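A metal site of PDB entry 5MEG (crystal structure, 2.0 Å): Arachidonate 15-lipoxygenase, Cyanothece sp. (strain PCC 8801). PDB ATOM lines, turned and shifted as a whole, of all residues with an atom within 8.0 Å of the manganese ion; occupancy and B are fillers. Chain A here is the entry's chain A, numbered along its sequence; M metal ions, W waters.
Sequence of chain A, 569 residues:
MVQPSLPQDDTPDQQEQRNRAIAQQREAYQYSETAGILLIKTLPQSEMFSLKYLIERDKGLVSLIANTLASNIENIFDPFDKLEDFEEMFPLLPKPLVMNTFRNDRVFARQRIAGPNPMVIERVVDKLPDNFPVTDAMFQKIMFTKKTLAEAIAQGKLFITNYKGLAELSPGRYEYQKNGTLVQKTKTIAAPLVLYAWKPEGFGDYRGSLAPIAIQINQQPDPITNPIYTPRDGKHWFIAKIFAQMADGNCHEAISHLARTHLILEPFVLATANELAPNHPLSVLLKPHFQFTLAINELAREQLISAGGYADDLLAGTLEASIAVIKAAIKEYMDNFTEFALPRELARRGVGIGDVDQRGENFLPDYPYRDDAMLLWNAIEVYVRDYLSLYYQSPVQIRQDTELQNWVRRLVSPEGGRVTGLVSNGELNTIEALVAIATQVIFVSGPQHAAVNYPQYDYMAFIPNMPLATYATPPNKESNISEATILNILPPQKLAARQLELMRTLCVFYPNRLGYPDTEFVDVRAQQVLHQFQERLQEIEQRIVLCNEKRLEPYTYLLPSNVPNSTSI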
ATOM      1  N   HIS A 252       2.716   3.449  -8.292  1.00  0.00           N
ATOM      2  CA  HIS A 252       1.424   4.107  -8.136  1.00  0.00           C
ATOM      3  C   HIS A 252       0.736   4.282  -9.490  1.00  0.00           C
ATOM      4  O   HIS A 252      -0.413   3.855  -9.676  1.00  0.00           O
ATOM      5  CB  HIS A 252       1.582   5.466  -7.449  1.00  0.00           C
ATOM      6  CG  HIS A 252       0.343   6.306  -7.521  1.00  0.00           C
ATOM      7  ND1 HIS A 252       0.119   7.203  -8.551  1.00  0.00           N
ATOM      8  CD2 HIS A 252      -0.730   6.378  -6.709  1.00  0.00           C
ATOM      9  CE1 HIS A 252      -1.044   7.796  -8.359  1.00  0.00           C
ATOM     10  NE2 HIS A 252      -1.586   7.313  -7.242  1.00  0.00           N
ATOM     11  N   GLU A 253       1.420   4.922 -10.441  1.00  0.00           N
ATOM     12  CA  GLU A 253       0.759   5.257 -11.689  1.00  0.00           C
ATOM     13  C   GLU A 253       0.528   4.022 -12.551  1.00  0.00           C
ATOM     14  O   GLU A 253      -0.551   3.855 -13.136  1.00  0.00           O
ATOM     15  CB  GLU A 253       1.559   6.317 -12.467  1.00  0.00           C
ATOM     16  CG  GLU A 253       1.647   7.678 -11.786  1.00  0.00           C
ATOM     17  CD  GLU A 253       0.312   8.400 -11.687  1.00  0.00           C
ATOM     18  OE1 GLU A 253      -0.718   7.856 -12.152  1.00  0.00           O
ATOM     19  OE2 GLU A 253       0.279   9.541 -11.163  1.00  0.00           O
ATOM     20  N   HIS A 257      -2.915   3.005 -10.048  1.00  0.00           N
ATOM     21  CA  HIS A 257      -3.825   3.976 -10.654  1.00  0.00           C
ATOM     22  C   HIS A 257      -4.335   3.487 -12.006  1.00  0.00           C
ATOM     23  O   HIS A 257      -5.512   3.121 -12.143  1.00  0.00           O
ATOM     24  CB  HIS A 257      -3.160   5.343 -10.764  1.00  0.00           C
ATOM     25  CG  HIS A 257      -4.052   6.424 -11.269  1.00  0.00           C
ATOM     26  ND1 HIS A 257      -3.583   7.597 -11.812  1.00  0.00           N
ATOM     27  CD2 HIS A 257      -5.406   6.505 -11.316  1.00  0.00           C
ATOM     28  CE1 HIS A 257      -4.613   8.360 -12.174  1.00  0.00           C
ATOM     29  NE2 HIS A 257      -5.724   7.713 -11.882  1.00  0.00           N
ATOM     30  N   LEU A 258      -3.459   3.460 -13.018  1.00  0.00           N
ATOM     31  CA  LEU A 258      -3.872   3.090 -14.375  1.00  0.00           C
ATOM     32  C   LEU A 258      -4.413   1.666 -14.432  1.00  0.00           C
ATOM     33  O   LEU A 258      -5.535   1.435 -14.876  1.00  0.00           O
ATOM     34  CB  LEU A 258      -2.709   3.270 -15.341  1.00  0.00           C
ATOM     35  CG  LEU A 258      -2.336   4.708 -15.717  1.00  0.00           C
ATOM     36  CD1 LEU A 258      -1.183   4.718 -16.712  1.00  0.00           C
ATOM     37  CD2 LEU A 258      -3.548   5.440 -16.278  1.00  0.00           C
ATOM     38  N   THR A 261      -7.364   0.627 -11.362  1.00  0.00           N
ATOM     39  CA  THR A 261      -8.665   1.290 -11.328  1.00  0.00           C
ATOM     40  C   THR A 261      -9.173   1.449 -12.754  1.00  0.00           C
ATOM     41  O   THR A 261     -10.055   0.706 -13.184  1.00  0.00           O
ATOM     42  CB  THR A 261      -8.599   2.656 -10.617  1.00  0.00           C
ATOM     43  OG1 THR A 261      -7.682   3.513 -11.308  1.00  0.00           O
ATOM     44  CG2 THR A 261      -8.176   2.492  -9.160  1.00  0.00           C
ATOM     45  N   HIS A 262      -8.571   2.382 -13.496  1.00  0.00           N
ATOM     46  CA  HIS A 262      -9.025   2.725 -14.838  1.00  0.00           C
ATOM     47  C   HIS A 262      -9.199   1.479 -15.721  1.00  0.00           C
ATOM     48  O   HIS A 262     -10.291   1.225 -16.242  1.00  0.00           O
ATOM     49  CB  HIS A 262      -8.030   3.684 -15.491  1.00  0.00           C
ATOM     50  CG  HIS A 262      -8.133   5.098 -14.991  1.00  0.00           C
ATOM     51  ND1 HIS A 262      -8.974   6.029 -15.562  1.00  0.00           N
ATOM     52  CD2 HIS A 262      -7.491   5.742 -13.983  1.00  0.00           C
ATOM     53  CE1 HIS A 262      -8.849   7.182 -14.924  1.00  0.00           C
ATOM     54  NE2 HIS A 262      -7.954   7.034 -13.962  1.00  0.00           N
ATOM     55  N   ILE A 296     -12.617   8.718 -20.219  1.00  0.00           N
ATOM     56  CA  ILE A 296     -11.345   9.028 -19.576  1.00  0.00           C
ATOM     57  C   ILE A 296     -10.314   7.964 -19.888  1.00  0.00           C
ATOM     58  O   ILE A 296      -9.104   8.253 -19.921  1.00  0.00           O
ATOM     59  CB  ILE A 296     -11.529   9.230 -18.047  1.00  0.00           C
ATOM     60  CG1 ILE A 296     -10.300   9.915 -17.449  1.00  0.00           C
ATOM     61  CG2 ILE A 296     -11.763   7.908 -17.347  1.00  0.00           C
ATOM     62  CD1 ILE A 296     -10.047  11.324 -17.972  1.00  0.00           C
ATOM     63  N   ASN A 297     -10.752   6.722 -20.136  1.00  0.00           N
ATOM     64  CA  ASN A 297      -9.799   5.692 -20.527  1.00  0.00           C
ATOM     65  C   ASN A 297      -9.335   5.885 -21.967  1.00  0.00           C
ATOM     66  O   ASN A 297      -8.186   5.537 -22.306  1.00  0.00           O
ATOM     67  CB  ASN A 297     -10.396   4.297 -20.317  1.00  0.00           C
ATOM     68  CG  ASN A 297     -10.422   3.893 -18.849  1.00  0.00           C
ATOM     69  OD1 ASN A 297      -9.845   4.561 -17.996  1.00  0.00           O
ATOM     70  ND2 ASN A 297     -11.100   2.782 -18.562  1.00  0.00           N
ATOM     71  N   ALA A 300      -6.729   8.276 -21.540  1.00  0.00           N
ATOM     72  CA  ALA A 300      -5.532   7.610 -21.046  1.00  0.00           C
ATOM     73  C   ALA A 300      -4.763   6.958 -22.184  1.00  0.00           C
ATOM     74  O   ALA A 300      -3.545   7.058 -22.260  1.00  0.00           O
ATOM     75  CB  ALA A 300      -5.900   6.586 -19.977  1.00  0.00           C
ATOM     76  N   LEU A 304      -1.793   9.452 -22.230  1.00  0.00           N
ATOM     77  CA  LEU A 304      -0.938   8.895 -21.192  1.00  0.00           C
ATOM     78  C   LEU A 304      -0.034   7.796 -21.738  1.00  0.00           C
ATOM     79  O   LEU A 304       1.193   7.944 -21.743  1.00  0.00           O
ATOM     80  CB  LEU A 304      -1.787   8.364 -20.029  1.00  0.00           C
ATOM     81  CG  LEU A 304      -2.517   9.382 -19.160  1.00  0.00           C
ATOM     82  CD1 LEU A 304      -3.408   8.685 -18.154  1.00  0.00           C
ATOM     83  CD2 LEU A 304      -1.536  10.297 -18.449  1.00  0.00           C
ATOM     84  N   HIS A 449     -10.408   4.506  -6.678  1.00  0.00           N
ATOM     85  CA  HIS A 449      -9.870   5.478  -7.614  1.00  0.00           C
ATOM     86  C   HIS A 449      -9.721   6.852  -6.958  1.00  0.00           C
ATOM     87  O   HIS A 449      -8.786   7.589  -7.274  1.00  0.00           O
ATOM     88  CB  HIS A 449     -10.743   5.589  -8.853  1.00  0.00           C
ATOM     89  CG  HIS A 449     -10.316   6.682  -9.777  1.00  0.00           C
ATOM     90  ND1 HIS A 449     -10.985   7.880  -9.857  1.00  0.00           N
ATOM     91  CD2 HIS A 449      -9.254   6.779 -10.607  1.00  0.00           C
ATOM     92  CE1 HIS A 449     -10.373   8.670 -10.724  1.00  0.00           C
ATOM     93  NE2 HIS A 449      -9.315   8.031 -11.192  1.00  0.00           N
ATOM     94  N   ALA A 450     -10.637   7.213  -6.059  1.00  0.00           N
ATOM     95  CA  ALA A 450     -10.471   8.479  -5.339  1.00  0.00           C
ATOM     96  C   ALA A 450      -9.193   8.449  -4.514  1.00  0.00           C
ATOM     97  O   ALA A 450      -8.393   9.402  -4.537  1.00  0.00           O
ATOM     98  CB  ALA A 450     -11.685   8.760  -4.464  1.00  0.00           C
ATOM     99  N   VAL A 452      -6.435   6.724  -4.824  1.00  0.00           N
ATOM    100  CA  VAL A 452      -5.159   6.766  -5.545  1.00  0.00           C
ATOM    101  C   VAL A 452      -5.053   7.948  -6.503  1.00  0.00           C
ATOM    102  O   VAL A 452      -3.946   8.275  -6.943  1.00  0.00           O
ATOM    103  CB  VAL A 452      -4.889   5.448  -6.290  1.00  0.00           C
ATOM    104  CG1 VAL A 452      -4.842   4.273  -5.303  1.00  0.00           C
ATOM    105  CG2 VAL A 452      -5.926   5.210  -7.375  1.00  0.00           C
ATOM    106  N   ASN A 453      -6.167   8.599  -6.832  1.00  0.00           N
ATOM    107  CA  ASN A 453      -6.166   9.664  -7.818  1.00  0.00           C
ATOM    108  C   ASN A 453      -5.983  11.039  -7.164  1.00  0.00           C
ATOM    109  O   ASN A 453      -5.126  11.811  -7.583  1.00  0.00           O
ATOM    110  CB  ASN A 453      -7.467   9.620  -8.635  1.00  0.00           C
ATOM    111  CG  ASN A 453      -7.453  10.587  -9.825  1.00  0.00           C
ATOM    112  OD1 ASN A 453      -7.163  10.191 -10.959  1.00  0.00           O
ATOM    113  ND2 ASN A 453      -7.775  11.849  -9.570  1.00  0.00           N
ATOM    114  N   TYR A 454      -6.755  11.332  -6.123  1.00  0.00           N
ATOM    115  CA  TYR A 454      -6.745  12.726  -5.665  1.00  0.00           C
ATOM    116  C   TYR A 454      -5.584  13.119  -4.747  1.00  0.00           C
ATOM    117  O   TYR A 454      -5.341  14.324  -4.584  1.00  0.00           O
ATOM    118  CB  TYR A 454      -8.093  13.044  -5.003  1.00  0.00           C
ATOM    119  CG  TYR A 454      -9.172  13.256  -6.047  1.00  0.00           C
ATOM    120  CD1 TYR A 454      -9.256  14.460  -6.742  1.00  0.00           C
ATOM    121  CD2 TYR A 454     -10.070  12.246  -6.357  1.00  0.00           C
ATOM    122  CE1 TYR A 454     -10.229  14.661  -7.704  1.00  0.00           C
ATOM    123  CE2 TYR A 454     -11.054  12.438  -7.323  1.00  0.00           C
ATOM    124  CZ  TYR A 454     -11.125  13.650  -7.991  1.00  0.00           C
ATOM    125  OH  TYR A 454     -12.087  13.858  -8.949  1.00  0.00           O
ATOM    126  N   GLN A 456      -2.671  12.761  -5.770  1.00  0.00           N
ATOM    127  CA  GLN A 456      -1.616  12.963  -6.752  1.00  0.00           C
ATOM    128  C   GLN A 456      -1.071  14.382  -6.724  1.00  0.00           C
ATOM    129  O   GLN A 456       0.133  14.584  -6.894  1.00  0.00           O
ATOM    130  CB  GLN A 456      -2.138  12.631  -8.148  1.00  0.00           C
ATOM    131  CG  GLN A 456      -2.070  11.168  -8.541  1.00  0.00           C
ATOM    132  CD  GLN A 456      -2.769  10.894  -9.855  1.00  0.00           C
ATOM    133  OE1 GLN A 456      -3.931  11.261 -10.039  1.00  0.00           O
ATOM    134  NE2 GLN A 456      -2.066  10.260 -10.783  1.00  0.00           N
ATOM    135  N   LEU A 506      -5.203  15.970 -13.395  1.00  0.00           N
ATOM    136  CA  LEU A 506      -5.869  14.799 -12.844  1.00  0.00           C
ATOM    137  C   LEU A 506      -6.628  15.091 -11.554  1.00  0.00           C
ATOM    138  O   LEU A 506      -7.499  14.299 -11.188  1.00  0.00           O
ATOM    139  CB  LEU A 506      -4.855  13.678 -12.596  1.00  0.00           C
ATOM    140  CG  LEU A 506      -4.075  13.157 -13.797  1.00  0.00           C
ATOM    141  CD1 LEU A 506      -3.232  11.950 -13.407  1.00  0.00           C
ATOM    142  CD2 LEU A 506      -5.009  12.821 -14.955  1.00  0.00           C
ATOM    143  N   CYS A 507      -6.328  16.195 -10.866  1.00  0.00           N
ATOM    144  CA  CYS A 507      -6.962  16.431  -9.575  1.00  0.00           C
ATOM    145  C   CYS A 507      -7.850  17.676  -9.526  1.00  0.00           C
ATOM    146  O   CYS A 507      -8.293  18.057  -8.434  1.00  0.00           O
ATOM    147  CB  CYS A 507      -5.893  16.543  -8.487  1.00  0.00           C
ATOM    148  SG  CYS A 507      -4.893  15.055  -8.315  1.00  0.00           S
ATOM    149  N   SER A 566     -17.809   7.638 -10.079  1.00  0.00           N
ATOM    150  CA  SER A 566     -17.185   6.789 -11.082  1.00  0.00           C
ATOM    151  C   SER A 566     -15.733   7.204 -11.264  1.00  0.00           C
ATOM    152  O   SER A 566     -15.345   8.326 -10.934  1.00  0.00           O
ATOM    153  CB  SER A 566     -17.919   6.869 -12.423  1.00  0.00           C
ATOM    154  OG  SER A 566     -17.778   8.152 -12.994  1.00  0.00           O
ATOM    155  N   THR A 567     -14.936   6.283 -11.787  1.00  0.00           N
ATOM    156  CA  THR A 567     -13.599   6.610 -12.262  1.00  0.00           C
ATOM    157  C   THR A 567     -13.746   7.442 -13.527  1.00  0.00           C
ATOM    158  O   THR A 567     -14.098   6.916 -14.594  1.00  0.00           O
ATOM    159  CB  THR A 567     -12.801   5.339 -12.510  1.00  0.00           C
ATOM    160  OG1 THR A 567     -12.567   4.661 -11.268  1.00  0.00           O
ATOM    161  CG2 THR A 567     -11.449   5.659 -13.167  1.00  0.00           C
ATOM    162  N   SER A 568     -13.489   8.742 -13.414  1.00  0.00           N
ATOM    163  CA  SER A 568     -13.835   9.642 -14.513  1.00  0.00           C
ATOM    164  C   SER A 568     -12.833  10.770 -14.719  1.00  0.00           C
ATOM    165  O   SER A 568     -13.155  11.728 -15.449  1.00  0.00           O
ATOM    166  CB  SER A 568     -15.225  10.221 -14.262  1.00  0.00           C
ATOM    167  OG  SER A 568     -15.365  10.616 -12.903  1.00  0.00           O
ATOM    168  N   ILE A 569     -11.652  10.707 -14.113  1.00  0.00           N
ATOM    169  CA  ILE A 569     -10.642  11.742 -14.286  1.00  0.00           C
ATOM    170  C   ILE A 569      -9.260  11.103 -14.087  1.00  0.00           C
ATOM    171  O   ILE A 569      -9.147  10.019 -13.521  1.00  0.00           O
ATOM    172  CB  ILE A 569     -10.869  12.919 -13.316  1.00  0.00           C
ATOM    173  CG1 ILE A 569     -10.002  14.117 -13.722  1.00  0.00           C
ATOM    174  CG2 ILE A 569     -10.583  12.506 -11.873  1.00  0.00           C
ATOM    175  CD1 ILE A 569     -10.189  15.336 -12.864  1.00  0.00           C
ATOM    176  OXT ILE A 569      -8.234  11.644 -14.503  1.00  0.00           O
HETATM  177 MN    MN M   1      -7.660   8.675 -12.494  1.00  0.00          MN
HETATM  178  O   HOH W   1      -6.327   9.926 -13.807  1.00  0.00           O
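The manganese ion is bound by a ring nitrogen (NE2) of His 449, the side-chain amide oxygen of Asn 453, a ring nitrogen (NE2) of His 262, a ring nitrogen (NE2) of His 257, water W1 and the chain-end carboxylate of Ile 569.
The backbone carbonyl oxygen (O) of Asn 453 lies close to the side-chain amide oxygen (OE1) of Gln 456 (2.8 Å). The side-chain amide nitrogen of Asn 453 is in hydrogen-bond range of the backbone carbonyl oxygen of Leu 506 (2.9 Å). O of Asn 453 sits at hydrogen-bond distance from SG of Cys 507 (3.3 Å). The backbone carbonyl oxygen (O) of His 262 is in hydrogen-bond range of the side-chain amide nitrogen (ND2) of Asn 297 (2.9 Å). A ring nitrogen (ND1) of His 257 sits at hydrogen-bond distance from the side-chain amide nitrogen (NE2) of Gln 456, at 3.2 Å. ND1 of His 257 sits at hydrogen-bond distance from OE1 of Glu 253 (2.9 Å). N of His 257 is in hydrogen-bond range of O of His 252 (2.7 Å).
Within 4 Å of the manganese ion: His 257, His 262, His 449, Asn 453 and Ile 569. The nearest printed residue that does not touch the manganese ion is Thr 567 (4.9 Å).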
